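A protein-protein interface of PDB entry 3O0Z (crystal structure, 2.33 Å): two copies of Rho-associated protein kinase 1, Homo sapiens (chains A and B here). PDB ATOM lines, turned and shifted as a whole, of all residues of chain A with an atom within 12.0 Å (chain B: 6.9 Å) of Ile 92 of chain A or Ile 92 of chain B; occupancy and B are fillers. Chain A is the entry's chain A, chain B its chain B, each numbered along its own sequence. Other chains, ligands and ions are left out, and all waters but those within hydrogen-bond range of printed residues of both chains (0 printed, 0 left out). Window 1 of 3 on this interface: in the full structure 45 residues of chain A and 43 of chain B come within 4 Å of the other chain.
O of Ile 92 of chain A is in hydrogen-bond range of NE2 of Gln 96 of chain A (3.3 Å).
Asp 88 of chain A touches Arg 85 of chain B, but with the chains exchanged Arg 85 of chain A does not touch Asp 88 of chain B (4.3 Å). Met 91 of chain A touches Ile 92 of chain B, and with the chains exchanged Ile 92 of chain A touches Met 91 of chain B. Leu 95 of chain A touches Ile 99 of chain B, and with the chains exchanged Ile 99 of chain A touches Leu 95 of chain B. Ile 99 of chain B touches its own counterpart, Ile 99 of chain A. Of the 12 pairs that touch across the chains among the printed residues, 7 have their exchanged pair printed and touching as well.
Of the printed residues of chain B, Ile 92 of chain A touches Asp 88, Met 91 and Ile 92. No residue of chain A comes within 4 Å of Gly 93 of chain B. Printed residues of chain B within 4 Å of Ile 99 of chain A: Leu 95 and Ile 99. Printed residues of chain A within 4 Å of Arg 85 of chain B: Asp 84 and Asp 88. Printed residues of chain A within 4 Å of Leu 95 of chain B: Leu 95 (3.9 Å) and Ile 99 (3.7 Å). Glu 90 of chain B touches none of the printed residues of chain A. The nearest printed residue of chain B that does not touch Ile 92 of chain A is Leu 95 of chain B (4.005 Å). The nearest printed residue of chain A that does not touch Ile 92 of chain B is Asp 88 of chain A (4.2 Å). The nearest printed residue of chain B that does not touch Leu 102 of chain A is Leu 95 of chain B (7.3 Å).
Met 91 of chain A touches Ile 92 of chain B. Ile 92 of chain A touches Asp 88 of chain B (CD1 to O, 3.9 Å). Ile 92 of chain A touches Met 91 of chain B. Ile 92 of chain A touches Ile 92 of chain B (CG1 to CG1, 3.4 Å). CD1 of Leu 95 of chain A touches CG2 of Ile 92 of chain B, at 3.7 Å. Leu 95 of chain A touches Leu 95 of chain B (CB to CB, 3.9 Å). Ile 99 of chain B touches Leu 95 of chain A (CD1 to CD2, 3.6 Å). CD1 of Ile 99 of chain A touches CD2 of Leu 95 of chain B (3.7 Å). Ile 99 of chain B touches Ile 99 of chain A. CD2 of Leu 102 of chain A touches O of Ile 99 of chain B (3.9 Å).
The side-chain carboxylate of Asp 88 of chain A is in salt-bridge range of the guanidinium group of Arg 85 of chain B (3.4 Å). The side-chain carboxylate (OD2) of Asp 84 of chain A is in salt-bridge range of the guanidinium group (NH1) of Arg 85 of chain B (3.6 Å).
Of the 13 printed residues of chain B, 6 touch a printed residue of chain A. Printed residues of chain B that touch a printed residue of chain A: Arg 85, Asp 88, Met 91, Ile 92, Leu 95 and Ile 99. Hydrophobic or aromatic side chains of chain B that line the printed part of chain A: Met 91, Ile 92, Leu 95 and Ile 99. Among the printed residues, 12 pairs touch across the chains. Among the printed residues, Asp or Glu carboxylates within 4 Å of a Lys or Arg side-chain nitrogen of the other chain: Asp 84 of chain A with Arg 85 of chain B and Asp 88 of chain A with Arg 85 of chain B.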
ATOM      1  N   GLU A  81     -21.611 -16.221  23.800  1.00  0.00           N
ATOM      2  CA  GLU A  81     -22.359 -15.477  22.784  1.00  0.00           C
ATOM      3  C   GLU A  81     -21.407 -14.562  22.058  1.00  0.00           C
ATOM      4  O   GLU A  81     -21.344 -14.574  20.845  1.00  0.00           O
ATOM      5  CB  GLU A  81     -23.435 -14.609  23.403  1.00  0.00           C
ATOM      6  CG  GLU A  81     -24.794 -14.705  22.764  1.00  0.00           C
ATOM      7  CD  GLU A  81     -25.861 -15.249  23.754  1.00  0.00           C
ATOM      8  OE1 GLU A  81     -26.927 -14.592  23.998  1.00  0.00           O
ATOM      9  OE2 GLU A  81     -25.610 -16.348  24.300  1.00  0.00           O
ATOM     10  N   ARG A  82     -20.668 -13.752  22.803  1.00  0.00           N
ATOM     11  CA  ARG A  82     -19.792 -12.782  22.168  1.00  0.00           C
ATOM     12  C   ARG A  82     -18.821 -13.444  21.182  1.00  0.00           C
ATOM     13  O   ARG A  82     -18.555 -12.909  20.104  1.00  0.00           O
ATOM     14  CB  ARG A  82     -19.060 -11.947  23.215  1.00  0.00           C
ATOM     15  CG  ARG A  82     -19.937 -10.851  23.831  1.00  0.00           C
ATOM     16  CD  ARG A  82     -19.256 -10.147  25.004  1.00  0.00           C
ATOM     17  NE  ARG A  82     -20.032  -8.982  25.448  1.00  0.00           N
ATOM     18  CZ  ARG A  82     -19.832  -8.325  26.594  1.00  0.00           C
ATOM     19  NH1 ARG A  82     -18.875  -8.711  27.442  1.00  0.00           N
ATOM     20  NH2 ARG A  82     -20.596  -7.276  26.895  1.00  0.00           N
ATOM     21  N   ARG A  83     -18.311 -14.612  21.557  1.00  0.00           N
ATOM     22  CA  ARG A  83     -17.398 -15.382  20.729  1.00  0.00           C
ATOM     23  C   ARG A  83     -18.071 -15.741  19.392  1.00  0.00           C
ATOM     24  O   ARG A  83     -17.447 -15.648  18.333  1.00  0.00           O
ATOM     25  CB  ARG A  83     -16.995 -16.658  21.461  1.00  0.00           C
ATOM     26  CG  ARG A  83     -16.060 -17.563  20.698  1.00  0.00           C
ATOM     27  CD  ARG A  83     -14.741 -17.630  21.439  1.00  0.00           C
ATOM     28  NE  ARG A  83     -14.345 -16.331  21.998  1.00  0.00           N
ATOM     29  CZ  ARG A  83     -13.552 -15.449  21.389  1.00  0.00           C
ATOM     30  NH1 ARG A  83     -13.059 -15.704  20.182  1.00  0.00           N
ATOM     31  NH2 ARG A  83     -13.249 -14.303  21.987  1.00  0.00           N
ATOM     32  N   ASP A  84     -19.342 -16.143  19.440  1.00  0.00           N
ATOM     33  CA  ASP A  84     -20.127 -16.383  18.233  1.00  0.00           C
ATOM     34  C   ASP A  84     -20.413 -15.110  17.429  1.00  0.00           C
ATOM     35  O   ASP A  84     -20.051 -15.043  16.244  1.00  0.00           O
ATOM     36  CB  ASP A  84     -21.419 -17.121  18.570  1.00  0.00           C
ATOM     37  CG  ASP A  84     -21.256 -18.622  18.498  1.00  0.00           C
ATOM     38  OD1 ASP A  84     -20.130 -19.069  18.785  1.00  0.00           O
ATOM     39  OD2 ASP A  84     -22.226 -19.344  18.152  1.00  0.00           O
ATOM     40  N   ARG A  85     -21.064 -14.107  18.034  1.00  0.00           N
ATOM     41  CA  ARG A  85     -21.228 -12.813  17.315  1.00  0.00           C
ATOM     42  C   ARG A  85     -19.919 -12.412  16.597  1.00  0.00           C
ATOM     43  O   ARG A  85     -19.941 -11.761  15.537  1.00  0.00           O
ATOM     44  CB  ARG A  85     -21.687 -11.648  18.213  1.00  0.00           C
ATOM     45  CG  ARG A  85     -23.117 -11.181  18.004  1.00  0.00           C
ATOM     46  CD  ARG A  85     -23.367  -9.792  18.665  1.00  0.00           C
ATOM     47  NE  ARG A  85     -23.023  -9.825  20.095  1.00  0.00           N
ATOM     48  CZ  ARG A  85     -23.714 -10.448  21.075  1.00  0.00           C
ATOM     49  NH1 ARG A  85     -24.876 -11.110  20.890  1.00  0.00           N
ATOM     50  NH2 ARG A  85     -23.273 -10.334  22.312  1.00  0.00           N
ATOM     51  N   GLY A  86     -18.790 -12.850  17.160  1.00  0.00           N
ATOM     52  CA  GLY A  86     -17.474 -12.606  16.592  1.00  0.00           C
ATOM     53  C   GLY A  86     -17.279 -13.365  15.280  1.00  0.00           C
ATOM     54  O   GLY A  86     -16.736 -12.820  14.323  1.00  0.00           O
ATOM     55  N   HIS A  87     -17.699 -14.624  15.237  1.00  0.00           N
ATOM     56  CA  HIS A  87     -17.569 -15.414  14.034  1.00  0.00           C
ATOM     57  C   HIS A  87     -18.453 -14.830  12.926  1.00  0.00           C
ATOM     58  O   HIS A  87     -18.076 -14.856  11.749  1.00  0.00           O
ATOM     59  CB  HIS A  87     -17.907 -16.885  14.299  1.00  0.00           C
ATOM     60  CG  HIS A  87     -17.002 -17.544  15.301  1.00  0.00           C
ATOM     61  ND1 HIS A  87     -17.348 -18.699  15.976  1.00  0.00           N
ATOM     62  CD2 HIS A  87     -15.769 -17.202  15.750  1.00  0.00           C
ATOM     63  CE1 HIS A  87     -16.366 -19.039  16.795  1.00  0.00           C
ATOM     64  NE2 HIS A  87     -15.397 -18.149  16.678  1.00  0.00           N
ATOM     65  N   ASP A  88     -19.613 -14.291  13.308  1.00  0.00           N
ATOM     66  CA  ASP A  88     -20.498 -13.590  12.372  1.00  0.00           C
ATOM     67  C   ASP A  88     -19.845 -12.352  11.755  1.00  0.00           C
ATOM     68  O   ASP A  88     -20.064 -12.039  10.583  1.00  0.00           O
ATOM     69  CB  ASP A  88     -21.811 -13.174  13.039  1.00  0.00           C
ATOM     70  CG  ASP A  88     -22.738 -14.353  13.328  1.00  0.00           C
ATOM     71  OD1 ASP A  88     -22.480 -15.476  12.841  1.00  0.00           O
ATOM     72  OD2 ASP A  88     -23.740 -14.142  14.053  1.00  0.00           O
ATOM     73  N   SER A  89     -19.044 -11.646  12.541  1.00  0.00           N
ATOM     74  CA  SER A  89     -18.321 -10.475  12.042  1.00  0.00           C
ATOM     75  C   SER A  89     -17.173 -10.848  11.104  1.00  0.00           C
ATOM     76  O   SER A  89     -16.815 -10.066  10.223  1.00  0.00           O
ATOM     77  CB  SER A  89     -17.784  -9.642  13.207  1.00  0.00           C
ATOM     78  OG  SER A  89     -18.874  -9.042  13.882  1.00  0.00           O
ATOM     79  N   GLU A  90     -16.588 -12.028  11.318  1.00  0.00           N
ATOM     80  CA  GLU A  90     -15.534 -12.517  10.463  1.00  0.00           C
ATOM     81  C   GLU A  90     -16.195 -12.860   9.155  1.00  0.00           C
ATOM     82  O   GLU A  90     -15.765 -12.418   8.105  1.00  0.00           O
ATOM     83  CB  GLU A  90     -14.907 -13.777  11.044  1.00  0.00           C
ATOM     84  CG  GLU A  90     -13.601 -13.552  11.783  1.00  0.00           C
ATOM     85  CD  GLU A  90     -13.075 -14.840  12.389  1.00  0.00           C
ATOM     86  OE1 GLU A  90     -12.903 -14.894  13.630  1.00  0.00           O
ATOM     87  OE2 GLU A  90     -12.860 -15.807  11.619  1.00  0.00           O
ATOM     88  N   MET A  91     -17.262 -13.644   9.245  1.00  0.00           N
ATOM     89  CA  MET A  91     -18.007 -14.071   8.073  1.00  0.00           C
ATOM     90  C   MET A  91     -18.497 -12.885   7.232  1.00  0.00           C
ATOM     91  O   MET A  91     -18.326 -12.861   6.019  1.00  0.00           O
ATOM     92  CB  MET A  91     -19.183 -14.954   8.488  1.00  0.00           C
ATOM     93  CG  MET A  91     -19.609 -15.897   7.388  1.00  0.00           C
ATOM     94  SD  MET A  91     -21.214 -16.883   7.793  1.00  0.00           S
ATOM     95  CE  MET A  91     -20.707 -17.514   9.589  1.00  0.00           C
ATOM     96  N   ILE A  92     -19.089 -11.887   7.880  1.00  0.00           N
ATOM     97  CA  ILE A  92     -19.592 -10.723   7.158  1.00  0.00           C
ATOM     98  C   ILE A  92     -18.448 -10.009   6.462  1.00  0.00           C
ATOM     99  O   ILE A  92     -18.569  -9.543   5.322  1.00  0.00           O
ATOM    100  CB  ILE A  92     -20.315  -9.761   8.102  1.00  0.00           C
ATOM    101  CG1 ILE A  92     -21.726 -10.258   8.370  1.00  0.00           C
ATOM    102  CG2 ILE A  92     -20.388  -8.368   7.516  1.00  0.00           C
ATOM    103  CD1 ILE A  92     -22.299  -9.632   9.641  1.00  0.00           C
ATOM    104  N   GLY A  93     -17.320  -9.939   7.150  1.00  0.00           N
ATOM    105  CA  GLY A  93     -16.123  -9.366   6.571  1.00  0.00           C
ATOM    106  C   GLY A  93     -15.623 -10.090   5.330  1.00  0.00           C
ATOM    107  O   GLY A  93     -15.147  -9.447   4.407  1.00  0.00           O
ATOM    108  N   ASP A  94     -15.711 -11.420   5.320  1.00  0.00           N
ATOM    109  CA  ASP A  94     -15.203 -12.213   4.209  1.00  0.00           C
ATOM    110  C   ASP A  94     -16.151 -12.169   3.024  1.00  0.00           C
ATOM    111  O   ASP A  94     -15.714 -12.112   1.881  1.00  0.00           O
ATOM    112  CB  ASP A  94     -14.954 -13.671   4.616  1.00  0.00           C
ATOM    113  CG  ASP A  94     -13.796 -13.818   5.591  1.00  0.00           C
ATOM    114  OD1 ASP A  94     -13.203 -12.779   5.980  1.00  0.00           O
ATOM    115  OD2 ASP A  94     -13.485 -14.975   5.971  1.00  0.00           O
ATOM    116  N   LEU A  95     -17.448 -12.203   3.289  1.00  0.00           N
ATOM    117  CA  LEU A  95     -18.421 -12.071   2.217  1.00  0.00           C
ATOM    118  C   LEU A  95     -18.249 -10.716   1.534  1.00  0.00           C
ATOM    119  O   LEU A  95     -18.213 -10.623   0.305  1.00  0.00           O
ATOM    120  CB  LEU A  95     -19.836 -12.238   2.759  1.00  0.00           C
ATOM    121  CG  LEU A  95     -20.080 -13.604   3.409  1.00  0.00           C
ATOM    122  CD1 LEU A  95     -21.366 -13.590   4.189  1.00  0.00           C
ATOM    123  CD2 LEU A  95     -20.129 -14.702   2.374  1.00  0.00           C
ATOM    124  N   GLN A  96     -18.116  -9.661   2.327  1.00  0.00           N
ATOM    125  CA  GLN A  96     -17.882  -8.321   1.773  1.00  0.00           C
ATOM    126  C   GLN A  96     -16.618  -8.241   0.922  1.00  0.00           C
ATOM    127  O   GLN A  96     -16.610  -7.602  -0.127  1.00  0.00           O
ATOM    128  CB  GLN A  96     -17.844  -7.250   2.875  1.00  0.00           C
ATOM    129  CG  GLN A  96     -19.226  -6.845   3.350  1.00  0.00           C
ATOM    130  CD  GLN A  96     -19.207  -6.176   4.714  1.00  0.00           C
ATOM    131  OE1 GLN A  96     -20.204  -5.586   5.134  1.00  0.00           O
ATOM    132  NE2 GLN A  96     -18.072  -6.261   5.412  1.00  0.00           N
ATOM    133  N   ALA A  97     -15.547  -8.875   1.379  1.00  0.00           N
ATOM    134  CA  ALA A  97     -14.311  -8.851   0.616  1.00  0.00           C
ATOM    135  C   ALA A  97     -14.449  -9.646  -0.668  1.00  0.00           C
ATOM    136  O   ALA A  97     -13.849  -9.302  -1.681  1.00  0.00           O
ATOM    137  CB  ALA A  97     -13.169  -9.403   1.426  1.00  0.00           C
ATOM    138  N   ARG A  98     -15.211 -10.730  -0.611  1.00  0.00           N
ATOM    139  CA  ARG A  98     -15.365 -11.592  -1.766  1.00  0.00           C
ATOM    140  C   ARG A  98     -16.198 -10.830  -2.794  1.00  0.00           C
ATOM    141  O   ARG A  98     -15.900 -10.849  -3.987  1.00  0.00           O
ATOM    142  CB  ARG A  98     -16.033 -12.918  -1.384  1.00  0.00           C
ATOM    143  CG  ARG A  98     -16.097 -13.917  -2.518  1.00  0.00           C
ATOM    144  CD  ARG A  98     -15.886 -15.344  -2.010  1.00  0.00           C
ATOM    145  NE  ARG A  98     -17.138 -16.082  -1.812  1.00  0.00           N
ATOM    146  CZ  ARG A  98     -17.522 -16.639  -0.660  1.00  0.00           C
ATOM    147  NH1 ARG A  98     -16.757 -16.548   0.429  1.00  0.00           N
ATOM    148  NH2 ARG A  98     -18.679 -17.294  -0.598  1.00  0.00           N
ATOM    149  N   ILE A  99     -17.218 -10.127  -2.312  1.00  0.00           N
ATOM    150  CA  ILE A  99     -18.073  -9.313  -3.157  1.00  0.00           C
ATOM    151  C   ILE A  99     -17.262  -8.271  -3.900  1.00  0.00           C
ATOM    152  O   ILE A  99     -17.338  -8.150  -5.124  1.00  0.00           O
ATOM    153  CB  ILE A  99     -19.119  -8.594  -2.333  1.00  0.00           C
ATOM    154  CG1 ILE A  99     -20.234  -9.563  -1.955  1.00  0.00           C
ATOM    155  CG2 ILE A  99     -19.678  -7.414  -3.105  1.00  0.00           C
ATOM    156  CD1 ILE A  99     -21.252  -8.958  -1.055  1.00  0.00           C
ATOM    157  N   THR A 100     -16.482  -7.512  -3.156  1.00  0.00           N
ATOM    158  CA  THR A 100     -15.595  -6.537  -3.771  1.00  0.00           C
ATOM    159  C   THR A 100     -14.730  -7.145  -4.888  1.00  0.00           C
ATOM    160  O   THR A 100     -14.576  -6.567  -5.966  1.00  0.00           O
ATOM    161  CB  THR A 100     -14.707  -5.905  -2.706  1.00  0.00           C
ATOM    162  OG1 THR A 100     -15.425  -4.827  -2.083  1.00  0.00           O
ATOM    163  CG2 THR A 100     -13.461  -5.377  -3.327  1.00  0.00           C
ATOM    164  N   SER A 101     -14.182  -8.322  -4.627  1.00  0.00           N
ATOM    165  CA  SER A 101     -13.309  -8.996  -5.571  1.00  0.00           C
ATOM    166  C   SER A 101     -14.086  -9.397  -6.851  1.00  0.00           C
ATOM    167  O   SER A 101     -13.679  -9.098  -7.987  1.00  0.00           O
ATOM    168  CB  SER A 101     -12.716 -10.229  -4.892  1.00  0.00           C
ATOM    169  OG  SER A 101     -11.673 -10.803  -5.654  1.00  0.00           O
ATOM    170  N   LEU A 102     -15.209 -10.068  -6.651  1.00  0.00           N
ATOM    171  CA  LEU A 102     -16.106 -10.416  -7.729  1.00  0.00           C
ATOM    172  C   LEU A 102     -16.483  -9.212  -8.585  1.00  0.00           C
ATOM    173  O   LEU A 102     -16.592  -9.326  -9.802  1.00  0.00           O
ATOM    174  CB  LEU A 102     -17.381 -11.016  -7.170  1.00  0.00           C
ATOM    175  CG  LEU A 102     -17.554 -12.527  -7.156  1.00  0.00           C
ATOM    176  CD1 LEU A 102     -16.227 -13.263  -7.131  1.00  0.00           C
ATOM    177  CD2 LEU A 102     -18.408 -12.851  -5.929  1.00  0.00           C
ATOM    178  N   ARG B  85     -27.602  -9.587  16.479  1.00  0.00           N
ATOM    179  CA  ARG B  85     -27.259 -10.855  15.836  1.00  0.00           C
ATOM    180  C   ARG B  85     -28.373 -11.269  14.884  1.00  0.00           C
ATOM    181  O   ARG B  85     -28.156 -12.029  13.941  1.00  0.00           O
ATOM    182  CB  ARG B  85     -26.996 -11.968  16.864  1.00  0.00           C
ATOM    183  CG  ARG B  85     -27.145 -13.387  16.282  1.00  0.00           C
ATOM    184  CD  ARG B  85     -26.086 -14.373  16.792  1.00  0.00           C
ATOM    185  NE  ARG B  85     -26.042 -15.616  16.016  1.00  0.00           N
ATOM    186  CZ  ARG B  85     -25.152 -16.593  16.190  1.00  0.00           C
ATOM    187  NH1 ARG B  85     -24.213 -16.489  17.120  1.00  0.00           N
ATOM    188  NH2 ARG B  85     -25.200 -17.678  15.423  1.00  0.00           N
ATOM    189  N   HIS B  87     -29.831  -9.021  13.166  1.00  0.00           N
ATOM    190  CA  HIS B  87     -29.484  -8.168  12.038  1.00  0.00           C
ATOM    191  C   HIS B  87     -28.292  -8.721  11.257  1.00  0.00           C
ATOM    192  O   HIS B  87     -28.337  -8.775  10.032  1.00  0.00           O
ATOM    193  CB  HIS B  87     -29.257  -6.722  12.488  1.00  0.00           C
ATOM    194  CG  HIS B  87     -30.507  -6.043  12.966  1.00  0.00           C
ATOM    195  ND1 HIS B  87     -31.604  -5.844  12.151  1.00  0.00           N
ATOM    196  CD2 HIS B  87     -30.835  -5.520  14.172  1.00  0.00           C
ATOM    197  CE1 HIS B  87     -32.553  -5.230  12.836  1.00  0.00           C
ATOM    198  NE2 HIS B  87     -32.113  -5.022  14.064  1.00  0.00           N
ATOM    199  N   ASP B  88     -27.250  -9.146  11.974  1.00  0.00           N
ATOM    200  CA  ASP B  88     -26.073  -9.773  11.374  1.00  0.00           C
ATOM    201  C   ASP B  88     -26.468 -10.940  10.453  1.00  0.00           C
ATOM    202  O   ASP B  88     -25.873 -11.148   9.385  1.00  0.00           O
ATOM    203  CB  ASP B  88     -25.087 -10.269  12.451  1.00  0.00           C
ATOM    204  CG  ASP B  88     -24.284  -9.127  13.109  1.00  0.00           C
ATOM    205  OD1 ASP B  88     -24.394  -7.967  12.639  1.00  0.00           O
ATOM    206  OD2 ASP B  88     -23.534  -9.396  14.092  1.00  0.00           O
ATOM    207  N   SER B  89     -27.474 -11.698  10.865  1.00  0.00           N
ATOM    208  CA  SER B  89     -27.857 -12.889  10.128  1.00  0.00           C
ATOM    209  C   SER B  89     -28.621 -12.573   8.842  1.00  0.00           C
ATOM    210  O   SER B  89     -28.482 -13.272   7.825  1.00  0.00           O
ATOM    211  CB  SER B  89     -28.658 -13.819  11.039  1.00  0.00           C
ATOM    212  OG  SER B  89     -29.367 -14.786  10.275  1.00  0.00           O
ATOM    213  N   GLU B  90     -29.424 -11.515   8.900  1.00  0.00           N
ATOM    214  CA  GLU B  90     -30.140 -10.990   7.740  1.00  0.00           C
ATOM    215  C   GLU B  90     -29.140 -10.465   6.706  1.00  0.00           C
ATOM    216  O   GLU B  90     -29.328 -10.641   5.497  1.00  0.00           O
ATOM    217  CB  GLU B  90     -31.064  -9.860   8.190  1.00  0.00           C
ATOM    218  CG  GLU B  90     -32.018  -9.309   7.152  1.00  0.00           C
ATOM    219  CD  GLU B  90     -33.109  -8.453   7.785  1.00  0.00           C
ATOM    220  OE1 GLU B  90     -33.722  -7.632   7.067  1.00  0.00           O
ATOM    221  OE2 GLU B  90     -33.348  -8.598   9.008  1.00  0.00           O
ATOM    222  N   MET B  91     -28.085  -9.813   7.197  1.00  0.00           N
ATOM    223  CA  MET B  91     -27.019  -9.312   6.338  1.00  0.00           C
ATOM    224  C   MET B  91     -26.284 -10.444   5.639  1.00  0.00           C
ATOM    225  O   MET B  91     -26.155 -10.447   4.416  1.00  0.00           O
ATOM    226  CB  MET B  91     -26.014  -8.511   7.149  1.00  0.00           C
ATOM    227  CG  MET B  91     -26.389  -7.071   7.367  1.00  0.00           C
ATOM    228  SD  MET B  91     -24.932  -6.214   8.312  1.00  0.00           S
ATOM    229  CE  MET B  91     -23.484  -6.809   7.183  1.00  0.00           C
ATOM    230  N   ILE B  92     -25.802 -11.406   6.419  1.00  0.00           N
ATOM    231  CA  ILE B  92     -25.053 -12.516   5.856  1.00  0.00           C
ATOM    232  C   ILE B  92     -25.835 -13.143   4.713  1.00  0.00           C
ATOM    233  O   ILE B  92     -25.263 -13.569   3.726  1.00  0.00           O
ATOM    234  CB  ILE B  92     -24.741 -13.563   6.915  1.00  0.00           C
ATOM    235  CG1 ILE B  92     -23.782 -12.988   7.951  1.00  0.00           C
ATOM    236  CG2 ILE B  92     -24.107 -14.790   6.305  1.00  0.00           C
ATOM    237  CD1 ILE B  92     -23.679 -13.858   9.175  1.00  0.00           C
ATOM    238  N   GLY B  93     -27.152 -13.169   4.847  1.00  0.00           N
ATOM    239  CA  GLY B  93     -28.001 -13.706   3.806  1.00  0.00           C
ATOM    240  C   GLY B  93     -27.988 -12.820   2.576  1.00  0.00           C
ATOM    241  O   GLY B  93     -27.888 -13.308   1.464  1.00  0.00           O
ATOM    242  N   ASP B  94     -28.081 -11.511   2.776  1.00  0.00           N
ATOM    243  CA  ASP B  94     -28.090 -10.574   1.658  1.00  0.00           C
ATOM    244  C   ASP B  94     -26.773 -10.609   0.876  1.00  0.00           C
ATOM    245  O   ASP B  94     -26.768 -10.535  -0.362  1.00  0.00           O
ATOM    246  CB  ASP B  94     -28.375  -9.152   2.152  1.00  0.00           C
ATOM    247  CG  ASP B  94     -29.777  -9.000   2.731  1.00  0.00           C
ATOM    248  OD1 ASP B  94     -30.623  -9.900   2.511  1.00  0.00           O
ATOM    249  OD2 ASP B  94     -30.030  -7.974   3.408  1.00  0.00           O
ATOM    250  N   LEU B  95     -25.661 -10.717   1.599  1.00  0.00           N
ATOM    251  CA  LEU B  95     -24.350 -10.695   0.966  1.00  0.00           C
ATOM    252  C   LEU B  95     -24.124 -12.016   0.265  1.00  0.00           C
ATOM    253  O   LEU B  95     -23.385 -12.093  -0.708  1.00  0.00           O
ATOM    254  CB  LEU B  95     -23.235 -10.467   1.975  1.00  0.00           C
ATOM    255  CG  LEU B  95     -23.324  -9.229   2.865  1.00  0.00           C
ATOM    256  CD1 LEU B  95     -22.349  -9.361   4.012  1.00  0.00           C
ATOM    257  CD2 LEU B  95     -23.053  -7.989   2.058  1.00  0.00           C
ATOM    258  N   GLN B  96     -24.751 -13.063   0.775  1.00  0.00           N
ATOM    259  CA  GLN B  96     -24.630 -14.348   0.137  1.00  0.00           C
ATOM    260  C   GLN B  96     -25.409 -14.361  -1.172  1.00  0.00           C
ATOM    261  O   GLN B  96     -25.060 -15.080  -2.110  1.00  0.00           O
ATOM    262  CB  GLN B  96     -25.126 -15.430   1.062  1.00  0.00           C
ATOM    263  CG  GLN B  96     -24.021 -16.123   1.783  1.00  0.00           C
ATOM    264  CD  GLN B  96     -24.547 -17.212   2.658  1.00  0.00           C
ATOM    265  OE1 GLN B  96     -25.716 -17.188   3.045  1.00  0.00           O
ATOM    266  NE2 GLN B  96     -23.704 -18.195   2.959  1.00  0.00           N
ATOM    267  N   ALA B  97     -26.459 -13.549  -1.226  1.00  0.00           N
ATOM    268  CA  ALA B  97     -27.269 -13.434  -2.425  1.00  0.00           C
ATOM    269  C   ALA B  97     -26.518 -12.606  -3.467  1.00  0.00           C
ATOM    270  O   ALA B  97     -26.449 -12.982  -4.647  1.00  0.00           O
ATOM    271  CB  ALA B  97     -28.624 -12.792  -2.099  1.00  0.00           C
ATOM    272  N   ILE B  99     -23.523 -12.338  -3.759  1.00  0.00           N
ATOM    273  CA  ILE B  99     -22.388 -13.098  -4.221  1.00  0.00           C
ATOM    274  C   ILE B  99     -22.758 -14.115  -5.285  1.00  0.00           C
ATOM    275  O   ILE B  99     -21.965 -14.373  -6.181  1.00  0.00           O
ATOM    276  CB  ILE B  99     -21.694 -13.796  -3.075  1.00  0.00           C
ATOM    277  CG1 ILE B  99     -20.840 -12.803  -2.303  1.00  0.00           C
ATOM    278  CG2 ILE B  99     -20.786 -14.934  -3.569  1.00  0.00           C
ATOM    279  CD1 ILE B  99     -20.303 -13.420  -1.013  1.00  0.00           C
